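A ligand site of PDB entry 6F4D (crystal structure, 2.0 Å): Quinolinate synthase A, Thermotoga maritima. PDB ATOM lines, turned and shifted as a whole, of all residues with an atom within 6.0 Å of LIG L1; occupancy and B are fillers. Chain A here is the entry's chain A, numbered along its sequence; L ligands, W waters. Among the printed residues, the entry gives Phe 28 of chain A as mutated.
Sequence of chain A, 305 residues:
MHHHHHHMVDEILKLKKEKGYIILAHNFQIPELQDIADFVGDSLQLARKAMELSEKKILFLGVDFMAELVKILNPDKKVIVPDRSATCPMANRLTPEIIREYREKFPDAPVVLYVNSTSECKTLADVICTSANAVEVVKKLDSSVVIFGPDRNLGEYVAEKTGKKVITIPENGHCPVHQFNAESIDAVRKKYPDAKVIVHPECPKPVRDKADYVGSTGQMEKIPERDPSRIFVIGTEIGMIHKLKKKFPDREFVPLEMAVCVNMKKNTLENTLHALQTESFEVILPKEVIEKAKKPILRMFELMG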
ATOM      1  N   HIS A  26      12.514  -4.971 -15.628  1.00  0.00           N
ATOM      2  CA  HIS A  26      11.578  -4.857 -14.524  1.00  0.00           C
ATOM      3  C   HIS A  26      10.445  -5.915 -14.663  1.00  0.00           C
ATOM      4  O   HIS A  26      10.115  -6.358 -15.759  1.00  0.00           O
ATOM      5  CB  HIS A  26      10.997  -3.450 -14.447  1.00  0.00           C
ATOM      6  CG  HIS A  26      10.109  -3.244 -13.263  1.00  0.00           C
ATOM      7  ND1 HIS A  26       8.743  -3.415 -13.323  1.00  0.00           N
ATOM      8  CD2 HIS A  26      10.405  -2.950 -11.983  1.00  0.00           C
ATOM      9  CE1 HIS A  26       8.228  -3.208 -12.125  1.00  0.00           C
ATOM     10  NE2 HIS A  26       9.223  -2.960 -11.280  1.00  0.00           N
ATOM     11  N   ASN A  27       9.861  -6.279 -13.516  1.00  0.00           N
ATOM     12  CA  ASN A  27       8.776  -7.237 -13.409  1.00  0.00           C
ATOM     13  C   ASN A  27       7.508  -6.935 -14.216  1.00  0.00           C
ATOM     14  O   ASN A  27       6.674  -7.842 -14.368  1.00  0.00           O
ATOM     15  CB  ASN A  27       8.370  -7.382 -11.922  1.00  0.00           C
ATOM     16  CG  ASN A  27       9.418  -8.082 -11.071  1.00  0.00           C
ATOM     17  OD1 ASN A  27      10.196  -8.887 -11.569  1.00  0.00           O
ATOM     18  ND2 ASN A  27       9.441  -7.780  -9.792  1.00  0.00           N
ATOM     19  N   PHE A  28       7.336  -5.715 -14.729  1.00  0.00           N
ATOM     20  CA  PHE A  28       6.160  -5.337 -15.496  1.00  0.00           C
ATOM     21  C   PHE A  28       6.344  -5.434 -16.996  1.00  0.00           C
ATOM     22  O   PHE A  28       5.398  -5.166 -17.752  1.00  0.00           O
ATOM     23  CB  PHE A  28       5.707  -3.920 -15.154  1.00  0.00           C
ATOM     24  CG  PHE A  28       5.270  -3.751 -13.739  1.00  0.00           C
ATOM     25  CD1 PHE A  28       5.073  -4.819 -12.863  1.00  0.00           C
ATOM     26  CD2 PHE A  28       5.006  -2.478 -13.273  1.00  0.00           C
ATOM     27  CE1 PHE A  28       4.654  -4.609 -11.558  1.00  0.00           C
ATOM     28  CE2 PHE A  28       4.593  -2.259 -11.982  1.00  0.00           C
ATOM     29  CZ  PHE A  28       4.416  -3.324 -11.118  1.00  0.00           C
ATOM     30  N   GLY A  41      13.662  -8.110 -12.006  1.00  0.00           N
ATOM     31  CA  GLY A  41      13.352  -7.838 -10.627  1.00  0.00           C
ATOM     32  C   GLY A  41      12.668  -6.528 -10.423  1.00  0.00           C
ATOM     33  O   GLY A  41      12.294  -5.852 -11.396  1.00  0.00           O
ATOM     34  N   ASP A  42      12.497  -6.171  -9.148  1.00  0.00           N
ATOM     35  CA  ASP A  42      11.867  -4.925  -8.786  1.00  0.00           C
ATOM     36  C   ASP A  42      12.881  -3.792  -8.834  1.00  0.00           C
ATOM     37  O   ASP A  42      14.040  -4.014  -9.231  1.00  0.00           O
ATOM     38  CB  ASP A  42      11.078  -5.052  -7.455  1.00  0.00           C
ATOM     39  CG  ASP A  42      11.940  -4.995  -6.209  1.00  0.00           C
ATOM     40  OD1 ASP A  42      13.181  -5.158  -6.304  1.00  0.00           O
ATOM     41  OD2 ASP A  42      11.311  -4.786  -5.108  1.00  0.00           O
ATOM     42  N   SER A  43      12.453  -2.584  -8.469  1.00  0.00           N
ATOM     43  CA  SER A  43      13.325  -1.405  -8.566  1.00  0.00           C
ATOM     44  C   SER A  43      14.543  -1.494  -7.649  1.00  0.00           C
ATOM     45  O   SER A  43      15.671  -1.231  -8.080  1.00  0.00           O
ATOM     46  CB  SER A  43      12.541  -0.111  -8.316  1.00  0.00           C
ATOM     47  OG  SER A  43      11.591   0.071  -9.354  1.00  0.00           O
ATOM     48  N   LEU A  44      14.313  -1.890  -6.400  1.00  0.00           N
ATOM     49  CA  LEU A  44      15.431  -2.081  -5.464  1.00  0.00           C
ATOM     50  C   LEU A  44      16.422  -3.138  -5.952  1.00  0.00           C
ATOM     51  O   LEU A  44      17.624  -2.914  -5.963  1.00  0.00           O
ATOM     52  CB  LEU A  44      14.940  -2.434  -4.064  1.00  0.00           C
ATOM     53  CG  LEU A  44      15.973  -2.609  -2.922  1.00  0.00           C
ATOM     54  CD1 LEU A  44      16.951  -1.426  -2.823  1.00  0.00           C
ATOM     55  CD2 LEU A  44      15.280  -2.790  -1.586  1.00  0.00           C
ATOM     56  N   PHE A  65      13.187   6.513 -15.695  1.00  0.00           N
ATOM     57  CA  PHE A  65      13.836   6.844 -14.431  1.00  0.00           C
ATOM     58  C   PHE A  65      14.744   5.701 -13.908  1.00  0.00           C
ATOM     59  O   PHE A  65      15.772   5.970 -13.292  1.00  0.00           O
ATOM     60  CB  PHE A  65      12.805   7.316 -13.366  1.00  0.00           C
ATOM     61  CG  PHE A  65      12.000   6.200 -12.782  1.00  0.00           C
ATOM     62  CD1 PHE A  65      12.547   5.346 -11.846  1.00  0.00           C
ATOM     63  CD2 PHE A  65      10.691   5.994 -13.174  1.00  0.00           C
ATOM     64  CE1 PHE A  65      11.797   4.304 -11.294  1.00  0.00           C
ATOM     65  CE2 PHE A  65       9.947   4.949 -12.651  1.00  0.00           C
ATOM     66  CZ  PHE A  65      10.498   4.104 -11.715  1.00  0.00           C
ATOM     67  N   CYS A  88       7.267   7.216 -16.497  1.00  0.00           N
ATOM     68  CA  CYS A  88       6.324   7.025 -15.402  1.00  0.00           C
ATOM     69  C   CYS A  88       5.594   8.337 -15.252  1.00  0.00           C
ATOM     70  O   CYS A  88       6.178   9.301 -14.788  1.00  0.00           O
ATOM     71  CB  CYS A  88       7.044   6.635 -14.119  1.00  0.00           C
ATOM     72  SG  CYS A  88       5.911   6.511 -12.723  1.00  0.00           S
ATOM     73  N   TYR A 114      10.737   9.072  -3.890  1.00  0.00           N
ATOM     74  CA  TYR A 114      10.524   7.737  -4.398  1.00  0.00           C
ATOM     75  C   TYR A 114      11.381   7.570  -5.651  1.00  0.00           C
ATOM     76  O   TYR A 114      11.561   8.532  -6.416  1.00  0.00           O
ATOM     77  CB  TYR A 114       9.035   7.554  -4.715  1.00  0.00           C
ATOM     78  CG  TYR A 114       8.568   6.156  -5.023  1.00  0.00           C
ATOM     79  CD1 TYR A 114       9.102   5.040  -4.379  1.00  0.00           C
ATOM     80  CD2 TYR A 114       7.511   5.937  -5.921  1.00  0.00           C
ATOM     81  CE1 TYR A 114       8.643   3.767  -4.649  1.00  0.00           C
ATOM     82  CE2 TYR A 114       7.042   4.667  -6.207  1.00  0.00           C
ATOM     83  CZ  TYR A 114       7.602   3.574  -5.575  1.00  0.00           C
ATOM     84  OH  TYR A 114       7.147   2.280  -5.827  1.00  0.00           O
ATOM     85  N   VAL A 115      11.910   6.365  -5.864  1.00  0.00           N
ATOM     86  CA  VAL A 115      12.754   6.111  -7.030  1.00  0.00           C
ATOM     87  C   VAL A 115      12.038   6.466  -8.345  1.00  0.00           C
ATOM     88  O   VAL A 115      12.668   6.822  -9.321  1.00  0.00           O
ATOM     89  CB  VAL A 115      13.274   4.655  -7.019  1.00  0.00           C
ATOM     90  CG1 VAL A 115      12.164   3.675  -7.360  1.00  0.00           C
ATOM     91  CG2 VAL A 115      14.451   4.488  -7.936  1.00  0.00           C
ATOM     92  N   ASN A 116      10.695   6.394  -8.367  1.00  0.00           N
ATOM     93  CA  ASN A 116       9.929   6.901  -9.498  1.00  0.00           C
ATOM     94  C   ASN A 116       9.918   8.431  -9.424  1.00  0.00           C
ATOM     95  O   ASN A 116       9.005   9.041  -8.889  1.00  0.00           O
ATOM     96  CB  ASN A 116       8.492   6.333  -9.520  1.00  0.00           C
ATOM     97  CG  ASN A 116       8.444   4.803  -9.570  1.00  0.00           C
ATOM     98  OD1 ASN A 116       9.046   4.106  -8.735  1.00  0.00           O
ATOM     99  ND2 ASN A 116       7.702   4.273 -10.539  1.00  0.00           N
ATOM    100  N   THR A 130      12.781   3.101  -2.403  1.00  0.00           N
ATOM    101  CA  THR A 130      11.811   2.289  -3.141  1.00  0.00           C
ATOM    102  C   THR A 130      10.741   1.852  -2.139  1.00  0.00           C
ATOM    103  O   THR A 130      10.874   2.112  -0.955  1.00  0.00           O
ATOM    104  CB  THR A 130      12.432   1.024  -3.771  1.00  0.00           C
ATOM    105  OG1 THR A 130      12.632   0.027  -2.768  1.00  0.00           O
ATOM    106  CG2 THR A 130      13.789   1.336  -4.435  1.00  0.00           C
ATOM    107  N   SER A 131       9.707   1.157  -2.620  1.00  0.00           N
ATOM    108  CA  SER A 131       8.587   0.741  -1.784  1.00  0.00           C
ATOM    109  C   SER A 131       9.027  -0.251  -0.723  1.00  0.00           C
ATOM    110  O   SER A 131       8.565  -0.171   0.399  1.00  0.00           O
ATOM    111  CB  SER A 131       7.474   0.152  -2.636  1.00  0.00           C
ATOM    112  OG  SER A 131       7.997  -0.785  -3.543  1.00  0.00           O
ATOM    113  N   ALA A 132       9.939  -1.139  -1.102  1.00  0.00           N
ATOM    114  CA  ALA A 132      10.558  -2.126  -0.230  1.00  0.00           C
ATOM    115  C   ALA A 132      11.227  -1.496   1.010  1.00  0.00           C
ATOM    116  O   ALA A 132      11.019  -1.946   2.132  1.00  0.00           O
ATOM    117  CB  ALA A 132      11.577  -2.932  -1.047  1.00  0.00           C
ATOM    118  N   CYS A 175      -0.231   6.567  -8.797  1.00  0.00           N
ATOM    119  CA  CYS A 175      -0.089   5.686  -9.938  1.00  0.00           C
ATOM    120  C   CYS A 175      -1.475   5.209 -10.352  1.00  0.00           C
ATOM    121  O   CYS A 175      -2.136   4.561  -9.544  1.00  0.00           O
ATOM    122  CB  CYS A 175       0.765   4.481  -9.558  1.00  0.00           C
ATOM    123  SG  CYS A 175       0.712   3.238 -10.829  1.00  0.00           S
ATOM    124  N   HIS A 178      -2.383   1.320 -10.136  1.00  0.00           N
ATOM    125  CA  HIS A 178      -2.607   0.703  -8.831  1.00  0.00           C
ATOM    126  C   HIS A 178      -3.875   1.218  -8.135  1.00  0.00           C
ATOM    127  O   HIS A 178      -4.104   0.903  -6.968  1.00  0.00           O
ATOM    128  CB  HIS A 178      -1.381   0.864  -7.927  1.00  0.00           C
ATOM    129  CG  HIS A 178      -0.264  -0.051  -8.303  1.00  0.00           C
ATOM    130  ND1 HIS A 178       0.708   0.308  -9.201  1.00  0.00           N
ATOM    131  CD2 HIS A 178       0.011  -1.323  -7.929  1.00  0.00           C
ATOM    132  CE1 HIS A 178       1.546  -0.704  -9.356  1.00  0.00           C
ATOM    133  NE2 HIS A 178       1.147  -1.708  -8.596  1.00  0.00           N
ATOM    134  N   HIS A 200       0.342  -3.658  -3.622  1.00  0.00           N
ATOM    135  CA  HIS A 200       1.433  -2.717  -3.594  1.00  0.00           C
ATOM    136  C   HIS A 200       1.108  -1.522  -2.740  1.00  0.00           C
ATOM    137  O   HIS A 200      -0.059  -1.101  -2.695  1.00  0.00           O
ATOM    138  CB  HIS A 200       1.714  -2.251  -5.014  1.00  0.00           C
ATOM    139  CG  HIS A 200       3.114  -1.775  -5.209  1.00  0.00           C
ATOM    140  ND1 HIS A 200       3.514  -0.511  -4.870  1.00  0.00           N
ATOM    141  CD2 HIS A 200       4.218  -2.424  -5.640  1.00  0.00           C
ATOM    142  CE1 HIS A 200       4.807  -0.391  -5.104  1.00  0.00           C
ATOM    143  NE2 HIS A 200       5.259  -1.548  -5.557  1.00  0.00           N
ATOM    144  N   GLU A 202       1.699   1.482  -3.437  1.00  0.00           N
ATOM    145  CA  GLU A 202       1.149   2.497  -4.334  1.00  0.00           C
ATOM    146  C   GLU A 202      -0.375   2.452  -4.420  1.00  0.00           C
ATOM    147  O   GLU A 202      -0.963   3.369  -4.957  1.00  0.00           O
ATOM    148  CB  GLU A 202       1.716   2.389  -5.758  1.00  0.00           C
ATOM    149  CG  GLU A 202       3.181   2.804  -5.895  1.00  0.00           C
ATOM    150  CD  GLU A 202       3.751   2.454  -7.253  1.00  0.00           C
ATOM    151  OE1 GLU A 202       2.982   2.399  -8.226  1.00  0.00           O
ATOM    152  OE2 GLU A 202       4.946   2.190  -7.361  1.00  0.00           O
ATOM    153  N   GLY A 215       3.326  -4.792  -0.046  1.00  0.00           N
ATOM    154  CA  GLY A 215       4.772  -4.768  -0.316  1.00  0.00           C
ATOM    155  C   GLY A 215       5.146  -4.505  -1.766  1.00  0.00           C
ATOM    156  O   GLY A 215       4.299  -4.572  -2.659  1.00  0.00           O
ATOM    157  N   SER A 216       6.414  -4.185  -1.978  1.00  0.00           N
ATOM    158  CA  SER A 216       7.025  -4.050  -3.319  1.00  0.00           C
ATOM    159  C   SER A 216       6.853  -5.336  -4.079  1.00  0.00           C
ATOM    160  O   SER A 216       6.601  -6.377  -3.495  1.00  0.00           O
ATOM    161  CB  SER A 216       8.538  -3.810  -3.207  1.00  0.00           C
ATOM    162  OG  SER A 216       9.244  -4.973  -2.790  1.00  0.00           O
ATOM    163  N   THR A 217       7.051  -5.292  -5.388  1.00  0.00           N
ATOM    164  CA  THR A 217       6.873  -6.503  -6.179  1.00  0.00           C
ATOM    165  C   THR A 217       7.943  -7.549  -5.808  1.00  0.00           C
ATOM    166  O   THR A 217       7.643  -8.748  -5.820  1.00  0.00           O
ATOM    167  CB  THR A 217       6.865  -6.260  -7.687  1.00  0.00           C
ATOM    168  OG1 THR A 217       8.136  -5.792  -8.111  1.00  0.00           O
ATOM    169  CG2 THR A 217       5.771  -5.269  -8.064  1.00  0.00           C
ATOM    170  N   GLY A 218       9.142  -7.086  -5.462  1.00  0.00           N
ATOM    171  CA  GLY A 218      10.214  -7.990  -4.976  1.00  0.00           C
ATOM    172  C   GLY A 218       9.771  -8.724  -3.689  1.00  0.00           C
ATOM    173  O   GLY A 218       9.986  -9.922  -3.526  1.00  0.00           O
ATOM    174  N   THR A 236      -1.152  -5.635  -8.227  1.00  0.00           N
ATOM    175  CA  THR A 236      -0.148  -4.855  -8.913  1.00  0.00           C
ATOM    176  C   THR A 236      -0.318  -5.053 -10.417  1.00  0.00           C
ATOM    177  O   THR A 236      -1.339  -5.634 -10.865  1.00  0.00           O
ATOM    178  CB  THR A 236       1.298  -5.179  -8.451  1.00  0.00           C
ATOM    179  OG1 THR A 236       2.220  -4.182  -8.924  1.00  0.00           O
ATOM    180  CG2 THR A 236       1.762  -6.553  -8.934  1.00  0.00           C
ATOM    181  N   MET A 264       5.144   0.603 -19.562  1.00  0.00           N
ATOM    182  CA  MET A 264       5.924  -0.609 -19.444  1.00  0.00           C
ATOM    183  C   MET A 264       5.790  -1.526 -20.661  1.00  0.00           C
ATOM    184  O   MET A 264       6.743  -2.247 -21.015  1.00  0.00           O
ATOM    185  CB  MET A 264       5.526  -1.326 -18.157  1.00  0.00           C
ATOM    186  CG  MET A 264       6.065  -0.662 -16.905  1.00  0.00           C
ATOM    187  SD  MET A 264       7.816  -1.082 -16.746  1.00  0.00           S
ATOM    188  CE  MET A 264       8.099  -0.711 -15.011  1.00  0.00           C
HETATM  189  C1  LIG L   1       6.253   0.058  -9.666  1.00  0.00           C
HETATM  190  C2  LIG L   1       6.519  -1.003  -8.641  1.00  0.00           C
HETATM  191  N1  LIG L   1       4.978   0.174  -9.921  1.00  0.00           N
HETATM  192  O1  LIG L   1       4.453   1.435 -10.078  1.00  0.00           O
HETATM  193  O2  LIG L   1       7.127   0.787 -10.117  1.00  0.00           O
HETATM  194  O3  LIG L   1       7.812  -0.848  -8.072  1.00  0.00           O
HETATM  195  O4  LIG L   1       7.644  -2.632  -6.423  1.00  0.00           O
HETATM  196  O5  LIG L   1       9.876  -1.558  -7.041  1.00  0.00           O
HETATM  197  O6  LIG L   1       8.675  -3.051  -8.701  1.00  0.00           O
HETATM  198  P1  LIG L   1       8.561  -2.135  -7.501  1.00  0.00           P
HETATM  199 FE1  LG2 L   2       2.541   3.120 -12.078  1.00  0.00          FE
HETATM  200 FE2  LG2 L   2       3.777   2.488 -14.477  1.00  0.00          FE
HETATM  201 FE3  LG2 L   2       5.079   1.913 -11.914  1.00  0.00          FE
HETATM  202 FE4  LG2 L   2       4.744   4.542 -12.917  1.00  0.00          FE
HETATM  203  S1  LG2 L   2       5.983   2.955 -13.931  1.00  0.00           S
HETATM  204  S2  LG2 L   2       4.305   3.784 -10.732  1.00  0.00           S
HETATM  205  S3  LG2 L   2       2.617   4.461 -13.942  1.00  0.00           S
HETATM  206  S4  LG2 L   2       3.074   1.014 -12.789  1.00  0.00           S
HETATM  207  O   HOH W   1       9.585   1.493  -8.920  1.00  0.00           O
HETATM  208  O   HOH W   2       9.233   0.567  -5.533  1.00  0.00           O
HETATM  209  O   HOH W   3      11.469  -2.082  -5.171  1.00  0.00           O
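An oxygen (O1) of LIG L1 binds an iron atom (FE3) of LG2 L2.
CE2 of Phe 28 touches N1 of LIG L1, at 3.2 Å.
CB of Asp 42 touches O6 of LIG L1, at 3.4 Å.
Tyr 114 touches LIG L1.
ND2 of Asn 116 touches O2 of LIG L1 (3.6 Å).
His 178 touches LIG L1.
Ser 216 touches LIG L1 (CA to O4, 3.5 Å).
12 residues have an atom within 4 Å of LIG L1: His 26, Phe 28, Asp 42, Ser 43, Tyr 114, Asn 116, Ser 131, His 178, His 200, Glu 202, Ser 216 and Thr 217.
The nearest printed residue that does not touch LIG L1 is Cys 175 (4.2 Å).
An iron atom (FE1) of LG2 L2 is bound by the side-chain sulfur of Cys 175.
OE2 of Glu 202 lies within hydrogen-bond range of N1 of LIG L1.
N of Ser 43 sits at hydrogen-bond distance from O5 of LIG L1.
FE4 of LG2 L2 is bound by SG of Cys 88, at 2.3 Å.
O4 of LIG L1 is in hydrogen-bond range of OG of Ser 131 (3.4 Å).
The side-chain amide nitrogen (ND2) of Asn 116 sits close to a sulfur (S2) of LG2 L2, at 3.4 Å.
An oxygen (O4) of LIG L1 sits at hydrogen-bond distance from a ring nitrogen (NE2) of His 200 (2.8 Å).
O6 of LIG L1 is in hydrogen-bond range of NE2 of His 26, 2.6 Å away.
An oxygen (O4) of LIG L1 is in hydrogen-bond range of the backbone NH of Thr 217 (2.9 Å).
An oxygen (O6) of LIG L1 lies within hydrogen-bond range of the side-chain hydroxyl of Thr 217, 2.9 Å away.
OG of Ser 43 lies close to O5 of LIG L1 (3.3 Å).
Water W3 lies within hydrogen-bond range of O5 of LIG L1, OD2 of Asp 42, N of Leu 44, OG1 of Thr 130 and N of Ser 43.
Water W2 lies within hydrogen-bond range of O5 of LIG L1, OG of Ser 131 and OH of Tyr 114.
Water W1 lies within hydrogen-bond range of OG of Ser 43 (2.5 Å), OD1 of Asn 116 (2.7 Å) and O2 of LIG L1 (2.8 Å).
OE2 of Glu 202 is in hydrogen-bond range of OH of Tyr 114, 2.7 Å away.
The side-chain carboxylate (OD2) of Asp 42 lies within hydrogen-bond range of the backbone NH (N) of Gly 218 (3.2 Å).
The side-chain sulfur of Cys 175 lies close to a ring nitrogen (ND1) of His 178, 3.4 Å away.
A ring nitrogen (NE2) of His 178 sits at hydrogen-bond distance from the side-chain hydroxyl of Thr 236 (2.7 Å).
The backbone NH of Glu 202 sits at hydrogen-bond distance from a ring nitrogen (ND1) of His 200 (3.1 Å).
The backbone NH of Leu 44 sits close to the side-chain carboxylate of Asp 42, at 3.5 Å.
The side-chain hydroxyl (OG) of Ser 216 sits close to the backbone NH (N) of Gly 218.
OG of Ser 216 lies within hydrogen-bond range of OD2 of Asp 42, at 3.1 Å.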
